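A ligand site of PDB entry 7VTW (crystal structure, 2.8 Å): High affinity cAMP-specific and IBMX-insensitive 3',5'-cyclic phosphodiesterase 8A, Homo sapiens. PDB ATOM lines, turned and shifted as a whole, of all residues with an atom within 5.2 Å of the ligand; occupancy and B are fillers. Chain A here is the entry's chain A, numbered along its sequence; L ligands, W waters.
A nitrogen (N5) of the ligand sits at hydrogen-bond distance from the side-chain amide oxygen (OD1) of Asn 248, 2.9 Å away. A nitrogen (N4) of the ligand lies within hydrogen-bond range of the side-chain hydroxyl (OH) of Tyr 74, at 3.2 Å.
ND2 of Asn 248 is in hydrogen-bond range of OH of Tyr 74 (2.7 Å). A ring nitrogen (ND1) of His 192 lies within hydrogen-bond range of the side-chain amino group (NZ) of Lys 242.
The backbone carbonyl oxygen (O) of Thr 187 sits close to a fluorine (F1) of the ligand (3.4 Å). SD of Met 189 sits close to O1 of the ligand (3.6 Å). A ring nitrogen (ND1) of His 192 lies close to a fluorine (F2) of the ligand, 3.3 Å away. Merely in contact with the ligand: Phe 300 (3.3 Å), Met 283 (3.4 Å), Phe 286 (3.4 Å), Gln 297 (3.5 Å), Tyr 267 (3.5 Å), Val 246 (3.5 Å), Phe 304 (3.6 Å), Ile 263 (3.7 Å) and Lys 242 (3.98 Å). Hydrophobic or aromatic side chains that line the ligand: Tyr 74, Met 189, His 192, Val 246, Ile 263, Met 283, Phe 286, Phe 300 and Phe 304. 14 residues have an atom within 4 Å of the ligand: Tyr 74, Thr 187, Met 189, His 192, Lys 242, Val 246, Asn 248, Ile 263, Tyr 267, Met 283, Phe 286, Gln 297, Phe 300 and Phe 304.
Water W1 lies within hydrogen-bond range of the side-chain carboxylate (OD2) of Asp 245 (3.0 Å) and the backbone carbonyl oxygen (O) of Thr 187 (3.0 Å).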
ATOM      1  N   TYR A  74      16.883  13.955  14.373  1.00  0.00           N
ATOM      2  CA  TYR A  74      17.627  12.995  13.548  1.00  0.00           C
ATOM      3  C   TYR A  74      18.203  11.850  14.386  1.00  0.00           C
ATOM      4  O   TYR A  74      17.802  10.702  14.212  1.00  0.00           O
ATOM      5  CB  TYR A  74      18.735  13.723  12.786  1.00  0.00           C
ATOM      6  CG  TYR A  74      19.417  12.904  11.717  1.00  0.00           C
ATOM      7  CD1 TYR A  74      18.899  12.841  10.419  1.00  0.00           C
ATOM      8  CD2 TYR A  74      20.591  12.201  11.989  1.00  0.00           C
ATOM      9  CE1 TYR A  74      19.537  12.107   9.428  1.00  0.00           C
ATOM     10  CE2 TYR A  74      21.230  11.457  10.999  1.00  0.00           C
ATOM     11  CZ  TYR A  74      20.701  11.415   9.729  1.00  0.00           C
ATOM     12  OH  TYR A  74      21.324  10.690   8.739  1.00  0.00           O
ATOM     13  N   THR A 187      32.981   5.958  12.395  1.00  0.00           N
ATOM     14  CA  THR A 187      31.944   6.927  12.006  1.00  0.00           C
ATOM     15  C   THR A 187      32.277   8.403  12.321  1.00  0.00           C
ATOM     16  O   THR A 187      31.551   9.296  11.860  1.00  0.00           O
ATOM     17  CB  THR A 187      30.587   6.586  12.644  1.00  0.00           C
ATOM     18  OG1 THR A 187      30.706   6.590  14.066  1.00  0.00           O
ATOM     19  CG2 THR A 187      30.095   5.220  12.177  1.00  0.00           C
ATOM     20  N   GLU A 188      33.333   8.663  13.090  1.00  0.00           N
ATOM     21  CA  GLU A 188      33.755  10.038  13.409  1.00  0.00           C
ATOM     22  C   GLU A 188      34.129  10.805  12.137  1.00  0.00           C
ATOM     23  O   GLU A 188      34.715  10.234  11.216  1.00  0.00           O
ATOM     24  CB  GLU A 188      34.932  10.029  14.404  1.00  0.00           C
ATOM     25  CG  GLU A 188      35.256  11.382  15.023  1.00  0.00           C
ATOM     26  CD  GLU A 188      36.592  11.414  15.749  1.00  0.00           C
ATOM     27  OE1 GLU A 188      37.176  10.347  16.015  1.00  0.00           O
ATOM     28  OE2 GLU A 188      37.057  12.531  16.068  1.00  0.00           O
ATOM     29  N   MET A 189      33.798  12.091  12.108  1.00  0.00           N
ATOM     30  CA  MET A 189      33.846  12.901  10.886  1.00  0.00           C
ATOM     31  C   MET A 189      35.267  13.190  10.380  1.00  0.00           C
ATOM     32  O   MET A 189      35.506  13.130   9.164  1.00  0.00           O
ATOM     33  CB  MET A 189      33.107  14.228  11.093  1.00  0.00           C
ATOM     34  CG  MET A 189      32.657  14.899   9.803  1.00  0.00           C
ATOM     35  SD  MET A 189      32.521  16.685   9.938  1.00  0.00           S
ATOM     36  CE  MET A 189      34.252  17.163   9.929  1.00  0.00           C
ATOM     37  N   HIS A 192      37.073  10.847   7.873  1.00  0.00           N
ATOM     38  CA  HIS A 192      36.352  10.555   6.619  1.00  0.00           C
ATOM     39  C   HIS A 192      37.316  10.233   5.470  1.00  0.00           C
ATOM     40  O   HIS A 192      37.257   9.154   4.900  1.00  0.00           O
ATOM     41  CB  HIS A 192      35.447  11.729   6.221  1.00  0.00           C
ATOM     42  CG  HIS A 192      34.711  11.533   4.930  1.00  0.00           C
ATOM     43  ND1 HIS A 192      33.368  11.210   4.879  1.00  0.00           N
ATOM     44  CD2 HIS A 192      35.125  11.626   3.640  1.00  0.00           C
ATOM     45  CE1 HIS A 192      32.997  11.094   3.612  1.00  0.00           C
ATOM     46  NE2 HIS A 192      34.037  11.350   2.849  1.00  0.00           N
ATOM     47  N   LYS A 242      30.333   3.446   7.416  1.00  0.00           N
ATOM     48  CA  LYS A 242      30.309   4.846   6.977  1.00  0.00           C
ATOM     49  C   LYS A 242      29.242   5.102   5.907  1.00  0.00           C
ATOM     50  O   LYS A 242      28.558   6.127   5.951  1.00  0.00           O
ATOM     51  CB  LYS A 242      31.678   5.290   6.455  1.00  0.00           C
ATOM     52  CG  LYS A 242      32.675   5.655   7.547  1.00  0.00           C
ATOM     53  CD  LYS A 242      34.084   5.849   7.010  1.00  0.00           C
ATOM     54  CE  LYS A 242      34.163   6.917   5.928  1.00  0.00           C
ATOM     55  NZ  LYS A 242      33.524   8.201   6.317  1.00  0.00           N
ATOM     56  N   ASP A 245      25.725   4.611   7.505  1.00  0.00           N
ATOM     57  CA  ASP A 245      25.384   5.737   8.367  1.00  0.00           C
ATOM     58  C   ASP A 245      24.737   6.880   7.577  1.00  0.00           C
ATOM     59  O   ASP A 245      23.665   7.349   7.934  1.00  0.00           O
ATOM     60  CB  ASP A 245      26.619   6.247   9.122  1.00  0.00           C
ATOM     61  CG  ASP A 245      26.295   7.329  10.145  1.00  0.00           C
ATOM     62  OD1 ASP A 245      25.190   7.312  10.734  1.00  0.00           O
ATOM     63  OD2 ASP A 245      27.161   8.206  10.373  1.00  0.00           O
ATOM     64  N   VAL A 246      25.406   7.291   6.497  1.00  0.00           N
ATOM     65  CA  VAL A 246      24.924   8.393   5.641  1.00  0.00           C
ATOM     66  C   VAL A 246      24.394   7.870   4.294  1.00  0.00           C
ATOM     67  O   VAL A 246      24.802   8.317   3.225  1.00  0.00           O
ATOM     68  CB  VAL A 246      25.988   9.495   5.465  1.00  0.00           C
ATOM     69  CG1 VAL A 246      26.222  10.217   6.781  1.00  0.00           C
ATOM     70  CG2 VAL A 246      27.307   8.952   4.917  1.00  0.00           C
ATOM     71  N   ASN A 248      21.112   8.119   3.615  1.00  0.00           N
ATOM     72  CA  ASN A 248      19.895   8.909   3.347  1.00  0.00           C
ATOM     73  C   ASN A 248      19.826   9.718   2.029  1.00  0.00           C
ATOM     74  O   ASN A 248      18.730   9.889   1.493  1.00  0.00           O
ATOM     75  CB  ASN A 248      19.499   9.790   4.556  1.00  0.00           C
ATOM     76  CG  ASN A 248      20.558  10.821   4.930  1.00  0.00           C
ATOM     77  OD1 ASN A 248      20.692  11.852   4.267  1.00  0.00           O
ATOM     78  ND2 ASN A 248      21.286  10.571   6.004  1.00  0.00           N
ATOM     79  N   PRO A 249      20.983  10.190   1.504  1.00  0.00           N
ATOM     80  CA  PRO A 249      20.925  10.806   0.162  1.00  0.00           C
ATOM     81  C   PRO A 249      20.703   9.798  -0.980  1.00  0.00           C
ATOM     82  O   PRO A 249      20.230  10.185  -2.048  1.00  0.00           O
ATOM     83  CB  PRO A 249      22.297  11.487   0.018  1.00  0.00           C
ATOM     84  CG  PRO A 249      22.860  11.532   1.397  1.00  0.00           C
ATOM     85  CD  PRO A 249      22.344  10.288   2.039  1.00  0.00           C
ATOM     86  N   TRP A 259      14.836  12.947   6.035  1.00  0.00           N
ATOM     87  CA  TRP A 259      16.134  12.911   6.724  1.00  0.00           C
ATOM     88  C   TRP A 259      16.869  14.253   6.677  1.00  0.00           C
ATOM     89  O   TRP A 259      17.538  14.633   7.635  1.00  0.00           O
ATOM     90  CB  TRP A 259      17.045  11.811   6.168  1.00  0.00           C
ATOM     91  CG  TRP A 259      16.598  10.404   6.506  1.00  0.00           C
ATOM     92  CD1 TRP A 259      16.303   9.413   5.619  1.00  0.00           C
ATOM     93  CD2 TRP A 259      16.412   9.851   7.809  1.00  0.00           C
ATOM     94  NE1 TRP A 259      15.943   8.268   6.295  1.00  0.00           N
ATOM     95  CE2 TRP A 259      16.000   8.511   7.643  1.00  0.00           C
ATOM     96  CE3 TRP A 259      16.556  10.351   9.115  1.00  0.00           C
ATOM     97  CZ2 TRP A 259      15.722   7.666   8.727  1.00  0.00           C
ATOM     98  CZ3 TRP A 259      16.284   9.505  10.190  1.00  0.00           C
ATOM     99  CH2 TRP A 259      15.871   8.182   9.987  1.00  0.00           C
ATOM    100  N   ALA A 260      16.741  14.963   5.553  1.00  0.00           N
ATOM    101  CA  ALA A 260      17.346  16.290   5.378  1.00  0.00           C
ATOM    102  C   ALA A 260      16.734  17.355   6.307  1.00  0.00           C
ATOM    103  O   ALA A 260      17.443  18.229   6.792  1.00  0.00           O
ATOM    104  CB  ALA A 260      17.232  16.748   3.926  1.00  0.00           C
ATOM    105  N   ILE A 263      18.030  16.368  10.217  1.00  0.00           N
ATOM    106  CA  ILE A 263      19.432  16.746  10.468  1.00  0.00           C
ATOM    107  C   ILE A 263      19.620  18.270  10.471  1.00  0.00           C
ATOM    108  O   ILE A 263      20.400  18.798  11.271  1.00  0.00           O
ATOM    109  CB  ILE A 263      20.400  16.063   9.453  1.00  0.00           C
ATOM    110  CG1 ILE A 263      21.851  16.137   9.954  1.00  0.00           C
ATOM    111  CG2 ILE A 263      20.279  16.637   8.054  1.00  0.00           C
ATOM    112  CD1 ILE A 263      22.203  15.110  11.011  1.00  0.00           C
ATOM    113  N   TYR A 267      20.770  20.794  13.650  1.00  0.00           N
ATOM    114  CA  TYR A 267      21.863  21.777  13.583  1.00  0.00           C
ATOM    115  C   TYR A 267      21.417  23.219  13.837  1.00  0.00           C
ATOM    116  O   TYR A 267      22.217  24.032  14.313  1.00  0.00           O
ATOM    117  CB  TYR A 267      22.597  21.705  12.229  1.00  0.00           C
ATOM    118  CG  TYR A 267      23.450  20.469  12.015  1.00  0.00           C
ATOM    119  CD1 TYR A 267      24.301  19.994  13.022  1.00  0.00           C
ATOM    120  CD2 TYR A 267      23.425  19.778  10.797  1.00  0.00           C
ATOM    121  CE1 TYR A 267      25.076  18.863  12.823  1.00  0.00           C
ATOM    122  CE2 TYR A 267      24.213  18.648  10.596  1.00  0.00           C
ATOM    123  CZ  TYR A 267      25.028  18.200  11.614  1.00  0.00           C
ATOM    124  OH  TYR A 267      25.815  17.083  11.448  1.00  0.00           O
ATOM    125  N   MET A 283      29.401  25.769  13.318  1.00  0.00           N
ATOM    126  CA  MET A 283      28.600  25.505  12.117  1.00  0.00           C
ATOM    127  C   MET A 283      27.762  26.750  11.765  1.00  0.00           C
ATOM    128  O   MET A 283      26.561  26.785  12.040  1.00  0.00           O
ATOM    129  CB  MET A 283      27.692  24.293  12.344  1.00  0.00           C
ATOM    130  CG  MET A 283      28.426  23.034  12.758  1.00  0.00           C
ATOM    131  SD  MET A 283      27.545  21.528  12.299  1.00  0.00           S
ATOM    132  CE  MET A 283      28.003  21.404  10.578  1.00  0.00           C
ATOM    133  N   PHE A 286      24.669  26.447   8.974  1.00  0.00           N
ATOM    134  CA  PHE A 286      23.450  25.794   9.472  1.00  0.00           C
ATOM    135  C   PHE A 286      22.746  26.641  10.549  1.00  0.00           C
ATOM    136  O   PHE A 286      22.793  26.322  11.730  1.00  0.00           O
ATOM    137  CB  PHE A 286      23.759  24.392  10.016  1.00  0.00           C
ATOM    138  CG  PHE A 286      24.254  23.436   8.965  1.00  0.00           C
ATOM    139  CD1 PHE A 286      25.608  23.317   8.703  1.00  0.00           C
ATOM    140  CD2 PHE A 286      23.359  22.652   8.248  1.00  0.00           C
ATOM    141  CE1 PHE A 286      26.070  22.425   7.737  1.00  0.00           C
ATOM    142  CE2 PHE A 286      23.811  21.769   7.276  1.00  0.00           C
ATOM    143  CZ  PHE A 286      25.173  21.661   7.018  1.00  0.00           C
ATOM    144  N   GLN A 297      22.358  20.648   1.079  1.00  0.00           N
ATOM    145  CA  GLN A 297      22.406  19.224   0.702  1.00  0.00           C
ATOM    146  C   GLN A 297      23.263  18.963  -0.536  1.00  0.00           C
ATOM    147  O   GLN A 297      23.948  17.945  -0.617  1.00  0.00           O
ATOM    148  CB  GLN A 297      20.990  18.677   0.493  1.00  0.00           C
ATOM    149  CG  GLN A 297      20.171  18.561   1.767  1.00  0.00           C
ATOM    150  CD  GLN A 297      20.698  17.515   2.739  1.00  0.00           C
ATOM    151  OE1 GLN A 297      21.281  16.506   2.329  1.00  0.00           O
ATOM    152  NE2 GLN A 297      20.494  17.735   4.025  1.00  0.00           N
ATOM    153  N   PHE A 300      26.716  19.233   0.757  1.00  0.00           N
ATOM    154  CA  PHE A 300      26.937  18.007   1.541  1.00  0.00           C
ATOM    155  C   PHE A 300      27.217  16.792   0.662  1.00  0.00           C
ATOM    156  O   PHE A 300      28.128  16.014   0.957  1.00  0.00           O
ATOM    157  CB  PHE A 300      25.738  17.739   2.462  1.00  0.00           C
ATOM    158  CG  PHE A 300      25.858  16.474   3.274  1.00  0.00           C
ATOM    159  CD1 PHE A 300      26.729  16.411   4.347  1.00  0.00           C
ATOM    160  CD2 PHE A 300      25.113  15.349   2.952  1.00  0.00           C
ATOM    161  CE1 PHE A 300      26.852  15.252   5.097  1.00  0.00           C
ATOM    162  CE2 PHE A 300      25.227  14.188   3.696  1.00  0.00           C
ATOM    163  CZ  PHE A 300      26.097  14.135   4.769  1.00  0.00           C
ATOM    164  N   PHE A 304      31.216  15.103   0.704  1.00  0.00           N
ATOM    165  CA  PHE A 304      31.365  13.808   1.377  1.00  0.00           C
ATOM    166  C   PHE A 304      30.835  12.619   0.573  1.00  0.00           C
ATOM    167  O   PHE A 304      31.532  11.614   0.402  1.00  0.00           O
ATOM    168  CB  PHE A 304      30.650  13.832   2.733  1.00  0.00           C
ATOM    169  CG  PHE A 304      31.167  14.871   3.679  1.00  0.00           C
ATOM    170  CD1 PHE A 304      30.475  16.062   3.886  1.00  0.00           C
ATOM    171  CD2 PHE A 304      32.358  14.663   4.370  1.00  0.00           C
ATOM    172  CE1 PHE A 304      30.952  17.021   4.768  1.00  0.00           C
ATOM    173  CE2 PHE A 304      32.842  15.623   5.257  1.00  0.00           C
ATOM    174  CZ  PHE A 304      32.141  16.801   5.446  1.00  0.00           C
ATOM    175  N   MET A 308      32.574   9.025  -1.857  1.00  0.00           N
ATOM    176  CA  MET A 308      32.490   7.858  -0.972  1.00  0.00           C
ATOM    177  C   MET A 308      31.648   6.734  -1.595  1.00  0.00           C
ATOM    178  O   MET A 308      32.123   5.609  -1.737  1.00  0.00           O
ATOM    179  CB  MET A 308      31.895   8.257   0.388  1.00  0.00           C
ATOM    180  CG  MET A 308      31.735   7.102   1.379  1.00  0.00           C
ATOM    181  SD  MET A 308      31.546   7.617   3.098  1.00  0.00           S
ATOM    182  CE  MET A 308      30.019   8.566   3.023  1.00  0.00           C
HETATM  183  N1  LIG L   1      23.137  16.189   5.776  1.00  0.00           N
HETATM  184  C1  LIG L   1      24.174  12.681   8.255  1.00  0.00           C
HETATM  185  C2  LIG L   1      23.437  14.124   6.891  1.00  0.00           C
HETATM  186  C3  LIG L   1      22.795  14.895   5.904  1.00  0.00           C
HETATM  187  N2  LIG L   1      24.765  16.046   7.547  1.00  0.00           N
HETATM  188  C4  LIG L   1      24.397  14.757   7.657  1.00  0.00           C
HETATM  189  C5  LIG L   1      24.071  16.654   6.600  1.00  0.00           C
HETATM  190  N3  LIG L   1      24.881  13.817   8.524  1.00  0.00           N
HETATM  191  N4  LIG L   1      23.304  12.795   7.291  1.00  0.00           N
HETATM  192  N5  LIG L   1      21.862  14.420   5.080  1.00  0.00           N
HETATM  193  C6  LIG L   1      25.945  14.008   9.509  1.00  0.00           C
HETATM  194 CL1  LIG L   1      24.427  18.349   6.412  1.00  0.00          CL
HETATM  195  C7  LIG L   1      27.275  14.346   8.876  1.00  0.00           C
HETATM  196  C8  LIG L   1      28.053  13.352   8.308  1.00  0.00           C
HETATM  197  C9  LIG L   1      29.258  13.680   7.697  1.00  0.00           C
HETATM  198  C10 LIG L   1      29.700  14.993   7.652  1.00  0.00           C
HETATM  199  C11 LIG L   1      28.917  15.977   8.228  1.00  0.00           C
HETATM  200  C12 LIG L   1      27.710  15.669   8.838  1.00  0.00           C
HETATM  201  O1  LIG L   1      29.524  17.214   8.056  1.00  0.00           O
HETATM  202  C13 LIG L   1      28.859  18.431   8.515  1.00  0.00           C
HETATM  203  C14 LIG L   1      29.915  19.494   8.481  1.00  0.00           C
HETATM  204  O2  LIG L   1      30.203  12.918   7.047  1.00  0.00           O
HETATM  205  C15 LIG L   1      30.027  11.495   6.916  1.00  0.00           C
HETATM  206  C16 LIG L   1      30.979  10.940   8.045  1.00  0.00           C
HETATM  207  F1  LIG L   1      30.479  11.227   9.279  1.00  0.00           F
HETATM  208  F2  LIG L   1      32.190  11.562   7.985  1.00  0.00           F
HETATM  209  C17 LIG L   1      27.678  18.723   7.633  1.00  0.00           C
HETATM  210  O   HOH W   1      30.037   8.126   9.522  1.00  0.00           O
HETATM  211  O   HOH W   2      29.511  12.599  12.266  1.00  0.00           O
